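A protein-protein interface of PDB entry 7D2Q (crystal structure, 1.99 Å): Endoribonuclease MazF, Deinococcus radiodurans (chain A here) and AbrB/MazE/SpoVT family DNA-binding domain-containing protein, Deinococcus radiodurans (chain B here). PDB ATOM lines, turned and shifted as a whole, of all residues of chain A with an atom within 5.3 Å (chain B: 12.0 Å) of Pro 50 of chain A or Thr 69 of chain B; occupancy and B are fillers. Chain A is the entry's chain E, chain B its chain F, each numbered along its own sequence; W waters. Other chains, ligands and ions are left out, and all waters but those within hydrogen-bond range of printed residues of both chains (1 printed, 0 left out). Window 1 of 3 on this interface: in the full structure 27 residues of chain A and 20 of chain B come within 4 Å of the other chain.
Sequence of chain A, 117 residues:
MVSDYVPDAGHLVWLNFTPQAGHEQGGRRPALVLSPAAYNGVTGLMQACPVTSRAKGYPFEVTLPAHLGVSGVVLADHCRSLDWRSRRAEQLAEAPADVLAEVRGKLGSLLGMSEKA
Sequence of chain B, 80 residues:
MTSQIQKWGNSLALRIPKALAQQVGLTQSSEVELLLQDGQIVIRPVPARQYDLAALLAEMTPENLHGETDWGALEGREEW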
ATOM      1  N   ARG A  29     -22.044 -12.356  -3.600  1.00  0.00           N
ATOM      2  CA  ARG A  29     -21.069 -11.682  -2.668  1.00  0.00           C
ATOM      3  C   ARG A  29     -19.593 -12.065  -2.802  1.00  0.00           C
ATOM      4  O   ARG A  29     -19.278 -13.265  -2.818  1.00  0.00           O
ATOM      5  CB  ARG A  29     -21.520 -11.955  -1.228  1.00  0.00           C
ATOM      6  CG  ARG A  29     -21.004 -10.952  -0.216  1.00  0.00           C
ATOM      7  CD  ARG A  29     -21.143 -11.458   1.220  1.00  0.00           C
ATOM      8  NE  ARG A  29     -22.532 -11.628   1.654  1.00  0.00           N
ATOM      9  CZ  ARG A  29     -23.337 -10.611   1.956  1.00  0.00           C
ATOM     10  NH1 ARG A  29     -22.888  -9.369   1.862  1.00  0.00           N
ATOM     11  NH2 ARG A  29     -24.586 -10.829   2.344  1.00  0.00           N
ATOM     12  N   PRO A  30     -18.668 -11.100  -2.846  1.00  0.00           N
ATOM     13  CA  PRO A  30     -17.247 -11.454  -2.914  1.00  0.00           C
ATOM     14  C   PRO A  30     -16.676 -11.785  -1.545  1.00  0.00           C
ATOM     15  O   PRO A  30     -17.181 -11.349  -0.509  1.00  0.00           O
ATOM     16  CB  PRO A  30     -16.586 -10.196  -3.502  1.00  0.00           C
ATOM     17  CG  PRO A  30     -17.570  -9.079  -3.301  1.00  0.00           C
ATOM     18  CD  PRO A  30     -18.863  -9.643  -2.751  1.00  0.00           C
ATOM     19  N   ALA A  31     -15.609 -12.589  -1.556  1.00  0.00           N
ATOM     20  CA  ALA A  31     -14.958 -13.002  -0.319  1.00  0.00           C
ATOM     21  C   ALA A  31     -13.488 -13.286  -0.579  1.00  0.00           C
ATOM     22  O   ALA A  31     -13.107 -13.719  -1.670  1.00  0.00           O
ATOM     23  CB  ALA A  31     -15.619 -14.253   0.277  1.00  0.00           C
ATOM     24  N   LEU A  32     -12.675 -13.059   0.452  1.00  0.00           N
ATOM     25  CA  LEU A  32     -11.254 -13.382   0.438  1.00  0.00           C
ATOM     26  C   LEU A  32     -11.042 -14.751   1.084  1.00  0.00           C
ATOM     27  O   LEU A  32     -11.399 -14.956   2.245  1.00  0.00           O
ATOM     28  CB  LEU A  32     -10.449 -12.316   1.185  1.00  0.00           C
ATOM     29  CG  LEU A  32      -8.974 -12.628   1.311  1.00  0.00           C
ATOM     30  CD1 LEU A  32      -8.272 -12.599  -0.057  1.00  0.00           C
ATOM     31  CD2 LEU A  32      -8.324 -11.661   2.292  1.00  0.00           C
ATOM     32  N   ALA A  48     -13.333 -18.130   4.723  1.00  0.00           N
ATOM     33  CA  ALA A  48     -13.255 -16.909   3.932  1.00  0.00           C
ATOM     34  C   ALA A  48     -13.875 -15.756   4.699  1.00  0.00           C
ATOM     35  O   ALA A  48     -14.767 -15.952   5.534  1.00  0.00           O
ATOM     36  CB  ALA A  48     -13.966 -17.047   2.582  1.00  0.00           C
ATOM     37  N   CYS A  49     -13.391 -14.534   4.389  1.00  0.00           N
ATOM     38  CA  CYS A  49     -13.862 -13.273   4.932  1.00  0.00           C
ATOM     39  C   CYS A  49     -14.591 -12.466   3.863  1.00  0.00           C
ATOM     40  O   CYS A  49     -14.124 -12.375   2.719  1.00  0.00           O
ATOM     41  CB  CYS A  49     -12.716 -12.421   5.485  1.00  0.00           C
ATOM     42  SG  CYS A  49     -11.687 -13.262   6.621  1.00  0.00           S
ATOM     43  N   PRO A  50     -15.708 -11.841   4.225  1.00  0.00           N
ATOM     44  CA  PRO A  50     -16.500 -11.107   3.235  1.00  0.00           C
ATOM     45  C   PRO A  50     -15.846  -9.786   2.848  1.00  0.00           C
ATOM     46  O   PRO A  50     -15.143  -9.150   3.639  1.00  0.00           O
ATOM     47  CB  PRO A  50     -17.828 -10.869   3.965  1.00  0.00           C
ATOM     48  CG  PRO A  50     -17.417 -10.760   5.413  1.00  0.00           C
ATOM     49  CD  PRO A  50     -16.253 -11.711   5.589  1.00  0.00           C
ATOM     50  N   VAL A  51     -16.089  -9.376   1.604  1.00  0.00           N
ATOM     51  CA  VAL A  51     -15.687  -8.058   1.119  1.00  0.00           C
ATOM     52  C   VAL A  51     -16.913  -7.165   1.162  1.00  0.00           C
ATOM     53  O   VAL A  51     -18.002  -7.590   0.760  1.00  0.00           O
ATOM     54  CB  VAL A  51     -15.115  -8.140  -0.306  1.00  0.00           C
ATOM     55  CG1 VAL A  51     -14.783  -6.736  -0.844  1.00  0.00           C
ATOM     56  CG2 VAL A  51     -13.900  -9.046  -0.338  1.00  0.00           C
ATOM     57  N   THR A  52     -16.763  -5.941   1.670  1.00  0.00           N
ATOM     58  CA  THR A  52     -17.873  -4.999   1.655  1.00  0.00           C
ATOM     59  C   THR A  52     -17.428  -3.651   1.098  1.00  0.00           C
ATOM     60  O   THR A  52     -16.277  -3.241   1.253  1.00  0.00           O
ATOM     61  CB  THR A  52     -18.501  -4.806   3.060  1.00  0.00           C
ATOM     62  OG1 THR A  52     -19.527  -3.813   2.978  1.00  0.00           O
ATOM     63  CG2 THR A  52     -17.470  -4.364   4.096  1.00  0.00           C
ATOM     64  N   VAL A  73     -13.433  -3.287   1.346  1.00  0.00           N
ATOM     65  CA  VAL A  73     -12.595  -3.709   2.462  1.00  0.00           C
ATOM     66  C   VAL A  73     -12.979  -5.128   2.834  1.00  0.00           C
ATOM     67  O   VAL A  73     -14.141  -5.530   2.718  1.00  0.00           O
ATOM     68  CB  VAL A  73     -12.719  -2.787   3.702  1.00  0.00           C
ATOM     69  CG1 VAL A  73     -12.221  -1.384   3.384  1.00  0.00           C
ATOM     70  CG2 VAL A  73     -14.173  -2.744   4.202  1.00  0.00           C
ATOM     71  N   VAL A  74     -11.993  -5.882   3.282  1.00  0.00           N
ATOM     72  CA  VAL A  74     -12.213  -7.211   3.830  1.00  0.00           C
ATOM     73  C   VAL A  74     -12.518  -7.045   5.307  1.00  0.00           C
ATOM     74  O   VAL A  74     -11.853  -6.260   5.998  1.00  0.00           O
ATOM     75  CB  VAL A  74     -10.978  -8.103   3.612  1.00  0.00           C
ATOM     76  CG1 VAL A  74     -11.221  -9.511   4.149  1.00  0.00           C
ATOM     77  CG2 VAL A  74     -10.615  -8.152   2.124  1.00  0.00           C
ATOM     78  N   LEU A  75     -13.537  -7.749   5.791  1.00  0.00           N
ATOM     79  CA  LEU A  75     -13.860  -7.725   7.224  1.00  0.00           C
ATOM     80  C   LEU A  75     -13.159  -8.906   7.874  1.00  0.00           C
ATOM     81  O   LEU A  75     -13.673 -10.026   7.856  1.00  0.00           O
ATOM     82  CB  LEU A  75     -15.367  -7.784   7.451  1.00  0.00           C
ATOM     83  CG  LEU A  75     -16.148  -6.588   6.910  1.00  0.00           C
ATOM     84  CD1 LEU A  75     -17.608  -6.666   7.354  1.00  0.00           C
ATOM     85  CD2 LEU A  75     -15.513  -5.285   7.361  1.00  0.00           C
ATOM     86  N   HIS A  78     -14.963 -11.229  10.372  1.00  0.00           N
ATOM     87  CA  HIS A  78     -16.186 -11.893   9.924  1.00  0.00           C
ATOM     88  C   HIS A  78     -15.912 -13.196   9.178  1.00  0.00           C
ATOM     89  O   HIS A  78     -16.769 -13.666   8.425  1.00  0.00           O
ATOM     90  CB  HIS A  78     -16.999 -10.946   9.041  1.00  0.00           C
ATOM     91  CG  HIS A  78     -17.713  -9.883   9.813  1.00  0.00           C
ATOM     92  ND1 HIS A  78     -17.080  -9.089  10.747  1.00  0.00           N
ATOM     93  CD2 HIS A  78     -19.008  -9.491   9.803  1.00  0.00           C
ATOM     94  CE1 HIS A  78     -17.957  -8.255  11.280  1.00  0.00           C
ATOM     95  NE2 HIS A  78     -19.133  -8.479  10.724  1.00  0.00           N
ATOM     96  N   CYS A  79     -14.742 -13.785   9.377  1.00  0.00           N
ATOM     97  CA  CYS A  79     -14.388 -15.041   8.729  1.00  0.00           C
ATOM     98  C   CYS A  79     -15.362 -16.154   9.119  1.00  0.00           C
ATOM     99  O   CYS A  79     -15.872 -16.203  10.241  1.00  0.00           O
ATOM    100  CB  CYS A  79     -12.954 -15.419   9.118  1.00  0.00           C
ATOM    101  SG  CYS A  79     -12.122 -16.582   8.012  1.00  0.00           S
ATOM    102  N   ASN B  64     -18.925   2.463  14.143  1.00  0.00           N
ATOM    103  CA  ASN B  64     -18.235   1.817  13.035  1.00  0.00           C
ATOM    104  C   ASN B  64     -18.413   0.301  13.012  1.00  0.00           C
ATOM    105  O   ASN B  64     -17.695  -0.367  12.272  1.00  0.00           O
ATOM    106  CB  ASN B  64     -16.731   2.190  13.027  1.00  0.00           C
ATOM    107  CG  ASN B  64     -15.970   1.711  14.268  1.00  0.00           C
ATOM    108  OD1 ASN B  64     -16.385   0.786  14.961  1.00  0.00           O
ATOM    109  ND2 ASN B  64     -14.827   2.344  14.535  1.00  0.00           N
ATOM    110  N   LEU B  65     -19.357  -0.251  13.775  1.00  0.00           N
ATOM    111  CA  LEU B  65     -19.556  -1.692  13.815  1.00  0.00           C
ATOM    112  C   LEU B  65     -20.133  -2.216  12.499  1.00  0.00           C
ATOM    113  O   LEU B  65     -20.821  -1.506  11.765  1.00  0.00           O
ATOM    114  CB  LEU B  65     -20.486  -2.081  14.971  1.00  0.00           C
ATOM    115  CG  LEU B  65     -20.046  -1.653  16.369  1.00  0.00           C
ATOM    116  CD1 LEU B  65     -20.988  -2.208  17.420  1.00  0.00           C
ATOM    117  CD2 LEU B  65     -18.589  -2.058  16.644  1.00  0.00           C
ATOM    118  N   HIS B  66     -19.836  -3.479  12.211  1.00  0.00           N
ATOM    119  CA  HIS B  66     -20.407  -4.212  11.084  1.00  0.00           C
ATOM    120  C   HIS B  66     -21.110  -5.444  11.640  1.00  0.00           C
ATOM    121  O   HIS B  66     -20.450  -6.324  12.198  1.00  0.00           O
ATOM    122  CB  HIS B  66     -19.329  -4.662  10.094  1.00  0.00           C
ATOM    123  CG  HIS B  66     -18.617  -3.547   9.392  1.00  0.00           C
ATOM    124  ND1 HIS B  66     -18.966  -3.126   8.127  1.00  0.00           N
ATOM    125  CD2 HIS B  66     -17.543  -2.804   9.755  1.00  0.00           C
ATOM    126  CE1 HIS B  66     -18.148  -2.160   7.748  1.00  0.00           C
ATOM    127  NE2 HIS B  66     -17.277  -1.944   8.718  1.00  0.00           N
ATOM    128  N   GLY B  67     -22.422  -5.534  11.455  1.00  0.00           N
ATOM    129  CA  GLY B  67     -23.171  -6.692  11.916  1.00  0.00           C
ATOM    130  C   GLY B  67     -22.806  -7.965  11.158  1.00  0.00           C
ATOM    131  O   GLY B  67     -22.004  -7.972  10.223  1.00  0.00           O
ATOM    132  N   GLU B  68     -23.435  -9.068  11.574  1.00  0.00           N
ATOM    133  CA  GLU B  68     -23.144 -10.376  10.990  1.00  0.00           C
ATOM    134  C   GLU B  68     -23.425 -10.367   9.491  1.00  0.00           C
ATOM    135  O   GLU B  68     -24.466  -9.885   9.043  1.00  0.00           O
ATOM    136  CB  GLU B  68     -23.972 -11.471  11.685  1.00  0.00           C
ATOM    137  CG  GLU B  68     -23.542 -12.921  11.362  1.00  0.00           C
ATOM    138  CD  GLU B  68     -24.629 -13.975  11.675  1.00  0.00           C
ATOM    139  OE1 GLU B  68     -25.130 -14.620  10.721  1.00  0.00           O
ATOM    140  OE2 GLU B  68     -24.982 -14.161  12.865  1.00  0.00           O
ATOM    141  N   THR B  69     -22.478 -10.889   8.720  1.00  0.00           N
ATOM    142  CA  THR B  69     -22.627 -10.960   7.275  1.00  0.00           C
ATOM    143  C   THR B  69     -23.733 -11.936   6.908  1.00  0.00           C
ATOM    144  O   THR B  69     -23.768 -13.065   7.407  1.00  0.00           O
ATOM    145  CB  THR B  69     -21.315 -11.412   6.640  1.00  0.00           C
ATOM    146  OG1 THR B  69     -20.295 -10.457   6.947  1.00  0.00           O
ATOM    147  CG2 THR B  69     -21.477 -11.559   5.128  1.00  0.00           C
ATOM    148  N   ASP B  70     -24.637 -11.506   6.036  1.00  0.00           N
ATOM    149  CA  ASP B  70     -25.741 -12.367   5.626  1.00  0.00           C
ATOM    150  C   ASP B  70     -25.255 -13.319   4.545  1.00  0.00           C
ATOM    151  O   ASP B  70     -25.049 -12.912   3.398  1.00  0.00           O
ATOM    152  CB  ASP B  70     -26.923 -11.545   5.116  1.00  0.00           C
ATOM    153  CG  ASP B  70     -28.084 -12.423   4.656  1.00  0.00           C
ATOM    154  OD1 ASP B  70     -28.236 -13.542   5.202  1.00  0.00           O
ATOM    155  OD2 ASP B  70     -28.833 -11.996   3.747  1.00  0.00           O
ATOM    156  N   TRP B  71     -25.080 -14.589   4.900  1.00  0.00           N
ATOM    157  CA  TRP B  71     -24.796 -15.620   3.916  1.00  0.00           C
ATOM    158  C   TRP B  71     -26.030 -16.440   3.582  1.00  0.00           C
ATOM    159  O   TRP B  71     -25.913 -17.507   2.973  1.00  0.00           O
ATOM    160  CB  TRP B  71     -23.663 -16.517   4.412  1.00  0.00           C
ATOM    161  CG  TRP B  71     -22.337 -15.830   4.355  1.00  0.00           C
ATOM    162  CD1 TRP B  71     -21.602 -15.354   5.413  1.00  0.00           C
ATOM    163  CD2 TRP B  71     -21.599 -15.511   3.177  1.00  0.00           C
ATOM    164  NE1 TRP B  71     -20.437 -14.777   4.954  1.00  0.00           N
ATOM    165  CE2 TRP B  71     -20.415 -14.858   3.586  1.00  0.00           C
ATOM    166  CE3 TRP B  71     -21.823 -15.715   1.810  1.00  0.00           C
ATOM    167  CZ2 TRP B  71     -19.451 -14.422   2.677  1.00  0.00           C
ATOM    168  CZ3 TRP B  71     -20.862 -15.273   0.906  1.00  0.00           C
ATOM    169  CH2 TRP B  71     -19.690 -14.636   1.348  1.00  0.00           C
ATOM    170  N   GLY B  72     -27.211 -15.952   3.952  1.00  0.00           N
ATOM    171  CA  GLY B  72     -28.446 -16.667   3.744  1.00  0.00           C
ATOM    172  C   GLY B  72     -28.445 -17.999   4.465  1.00  0.00           C
ATOM    173  O   GLY B  72     -27.827 -18.176   5.521  1.00  0.00           O
ATOM    174  N   ALA B  73     -29.139 -18.961   3.866  1.00  0.00           N
ATOM    175  CA  ALA B  73     -29.322 -20.266   4.475  1.00  0.00           C
ATOM    176  C   ALA B  73     -28.022 -21.060   4.456  1.00  0.00           C
ATOM    177  O   ALA B  73     -27.124 -20.817   3.647  1.00  0.00           O
ATOM    178  CB  ALA B  73     -30.413 -21.052   3.741  1.00  0.00           C
ATOM    179  N   LEU B  74     -27.934 -22.025   5.368  1.00  0.00           N
ATOM    180  CA  LEU B  74     -26.825 -22.965   5.345  1.00  0.00           C
ATOM    181  C   LEU B  74     -26.888 -23.794   4.072  1.00  0.00           C
ATOM    182  O   LEU B  74     -27.969 -24.155   3.602  1.00  0.00           O
ATOM    183  CB  LEU B  74     -26.869 -23.861   6.579  1.00  0.00           C
ATOM    184  CG  LEU B  74     -26.896 -23.047   7.877  1.00  0.00           C
ATOM    185  CD1 LEU B  74     -26.905 -23.941   9.120  1.00  0.00           C
ATOM    186  CD2 LEU B  74     -25.724 -22.066   7.909  1.00  0.00           C
ATOM    187  N   GLU B  75     -25.723 -24.081   3.500  1.00  0.00           N
ATOM    188  CA  GLU B  75     -25.631 -24.790   2.233  1.00  0.00           C
ATOM    189  C   GLU B  75     -24.640 -25.933   2.360  1.00  0.00           C
ATOM    190  O   GLU B  75     -23.606 -25.796   3.018  1.00  0.00           O
ATOM    191  CB  GLU B  75     -25.191 -23.853   1.094  1.00  0.00           C
ATOM    192  CG  GLU B  75     -26.087 -22.639   0.888  1.00  0.00           C
ATOM    193  CD  GLU B  75     -26.172 -22.219  -0.570  1.00  0.00           C
ATOM    194  OE1 GLU B  75     -25.663 -22.974  -1.433  1.00  0.00           O
ATOM    195  OE2 GLU B  75     -26.744 -21.136  -0.855  1.00  0.00           O
ATOM    196  N   GLU B  78     -21.779 -27.126   5.112  1.00  0.00           N
ATOM    197  CA  GLU B  78     -21.785 -26.169   6.215  1.00  0.00           C
ATOM    198  C   GLU B  78     -22.608 -26.730   7.357  1.00  0.00           C
ATOM    199  O   GLU B  78     -23.801 -27.001   7.196  1.00  0.00           O
ATOM    200  CB  GLU B  78     -22.358 -24.823   5.763  1.00  0.00           C
ATOM    201  CG  GLU B  78     -21.427 -23.998   4.881  1.00  0.00           C
ATOM    202  CD  GLU B  78     -22.143 -22.899   4.110  1.00  0.00           C
ATOM    203  OE1 GLU B  78     -21.634 -22.506   3.044  1.00  0.00           O
ATOM    204  OE2 GLU B  78     -23.206 -22.418   4.566  1.00  0.00           O
ATOM    205  N   TRP B  80     -23.226 -25.354  10.440  1.00  0.00           N
ATOM    206  CA  TRP B  80     -24.018 -24.411  11.216  1.00  0.00           C
ATOM    207  C   TRP B  80     -23.850 -22.972  10.728  1.00  0.00           C
ATOM    208  O   TRP B  80     -24.306 -22.026  11.380  1.00  0.00           O
ATOM    209  CB  TRP B  80     -23.649 -24.517  12.699  1.00  0.00           C
ATOM    210  CG  TRP B  80     -22.348 -23.857  13.045  1.00  0.00           C
ATOM    211  CD1 TRP B  80     -21.244 -23.733  12.242  1.00  0.00           C
ATOM    212  CD2 TRP B  80     -22.013 -23.230  14.292  1.00  0.00           C
ATOM    213  NE1 TRP B  80     -20.247 -23.058  12.917  1.00  0.00           N
ATOM    214  CE2 TRP B  80     -20.694 -22.738  14.172  1.00  0.00           C
ATOM    215  CE3 TRP B  80     -22.703 -23.029  15.492  1.00  0.00           C
ATOM    216  CZ2 TRP B  80     -20.051 -22.072  15.208  1.00  0.00           C
ATOM    217  CZ3 TRP B  80     -22.067 -22.363  16.515  1.00  0.00           C
ATOM    218  CH2 TRP B  80     -20.752 -21.892  16.371  1.00  0.00           C
HETATM  219  O   HOH W   1     -19.144 -13.792   7.422  1.00  0.00           O
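Among the printed residues, merely in contact across the chains: Arg 29 of chain A with Thr 69 of chain B, Arg 29 of chain A with Trp 71 of chain B, Pro 50 of chain A with Thr 69 of chain B, Leu 75 of chain A with His 66 of chain B and His 78 of chain A with Thr 69 of chain B.
The backbone carbonyl oxygen (O) of Pro 50 of chain A lies within hydrogen-bond range of the backbone NH (N) of Leu 75 of chain A, at 3.0 Å.
OD1 of Asp 70 of chain B lies within hydrogen-bond range of N of Gly 72 of chain B (2.9 Å).
Of chain B, only Thr 69 (3.3 Å) comes within 4 Å of Pro 50 of chain A.
Of the printed residues of chain A, Thr 69 of chain B touches Arg 29, Pro 50 and His 78.
No residue of chain B comes within 4 Å of Pro 30 of chain A.
No residue of chain B comes within 4 Å of Ala 48 of chain A.
No residue of chain B comes within 4 Å of Cys 49 of chain A.
No residue of chain B comes within 4 Å of Val 51 of chain A.
Of chain B, only His 66 comes within 4 Å of Leu 75 of chain A.
No residue of chain B comes within 4 Å of Cys 79 of chain A.
Printed residues of chain A within 4 Å of Trp 71 of chain B: Arg 29 (3.5 Å).
Of the printed residues of chain A, Gly 67 of chain B touches His 78.
Of the printed residues of chain A, Asp 70 of chain B touches Arg 29 (2.4 Å).
Of the printed residues of chain B, Arg 29 of chain A touches Thr 69 (3.6 Å), Asp 70 (2.4 Å) and Trp 71 (3.5 Å).
The nearest residue of chain B that does not touch Pro 50 of chain A is Trp 71 of chain B (4.1 Å).
The nearest residue of chain A that does not touch Thr 69 of chain B is Leu 75 of chain A (4.7 Å).
The nearest printed residue of chain B that does not touch Arg 29 of chain A is Gly 72 of chain B (6.0 Å).
Water W1 bridges the backbone carbonyl oxygen of His 78 of chain A (2.6 Å) and the indole nitrogen of Trp 71 of chain B (3.0 Å).
Hydrophobic or aromatic side chains of chain A that line the printed part of chain B: Pro 50, Leu 75 and His 78.
Hydrophobic or aromatic side chains of chain B that line the printed part of chain A: His 66 and Trp 71.
NE of Arg 29 of chain A sits close to O of Asp 70 of chain B, at 3.3 Å.
The backbone carbonyl oxygen (O) of His 66 of chain B sits at hydrogen-bond distance from a ring nitrogen (NE2) of His 78 of chain A (2.9 Å).
A ring nitrogen (NE2) of His 78 of chain A is in hydrogen-bond range of the backbone carbonyl oxygen (O) of Gly 67 of chain B, at 3.0 Å.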
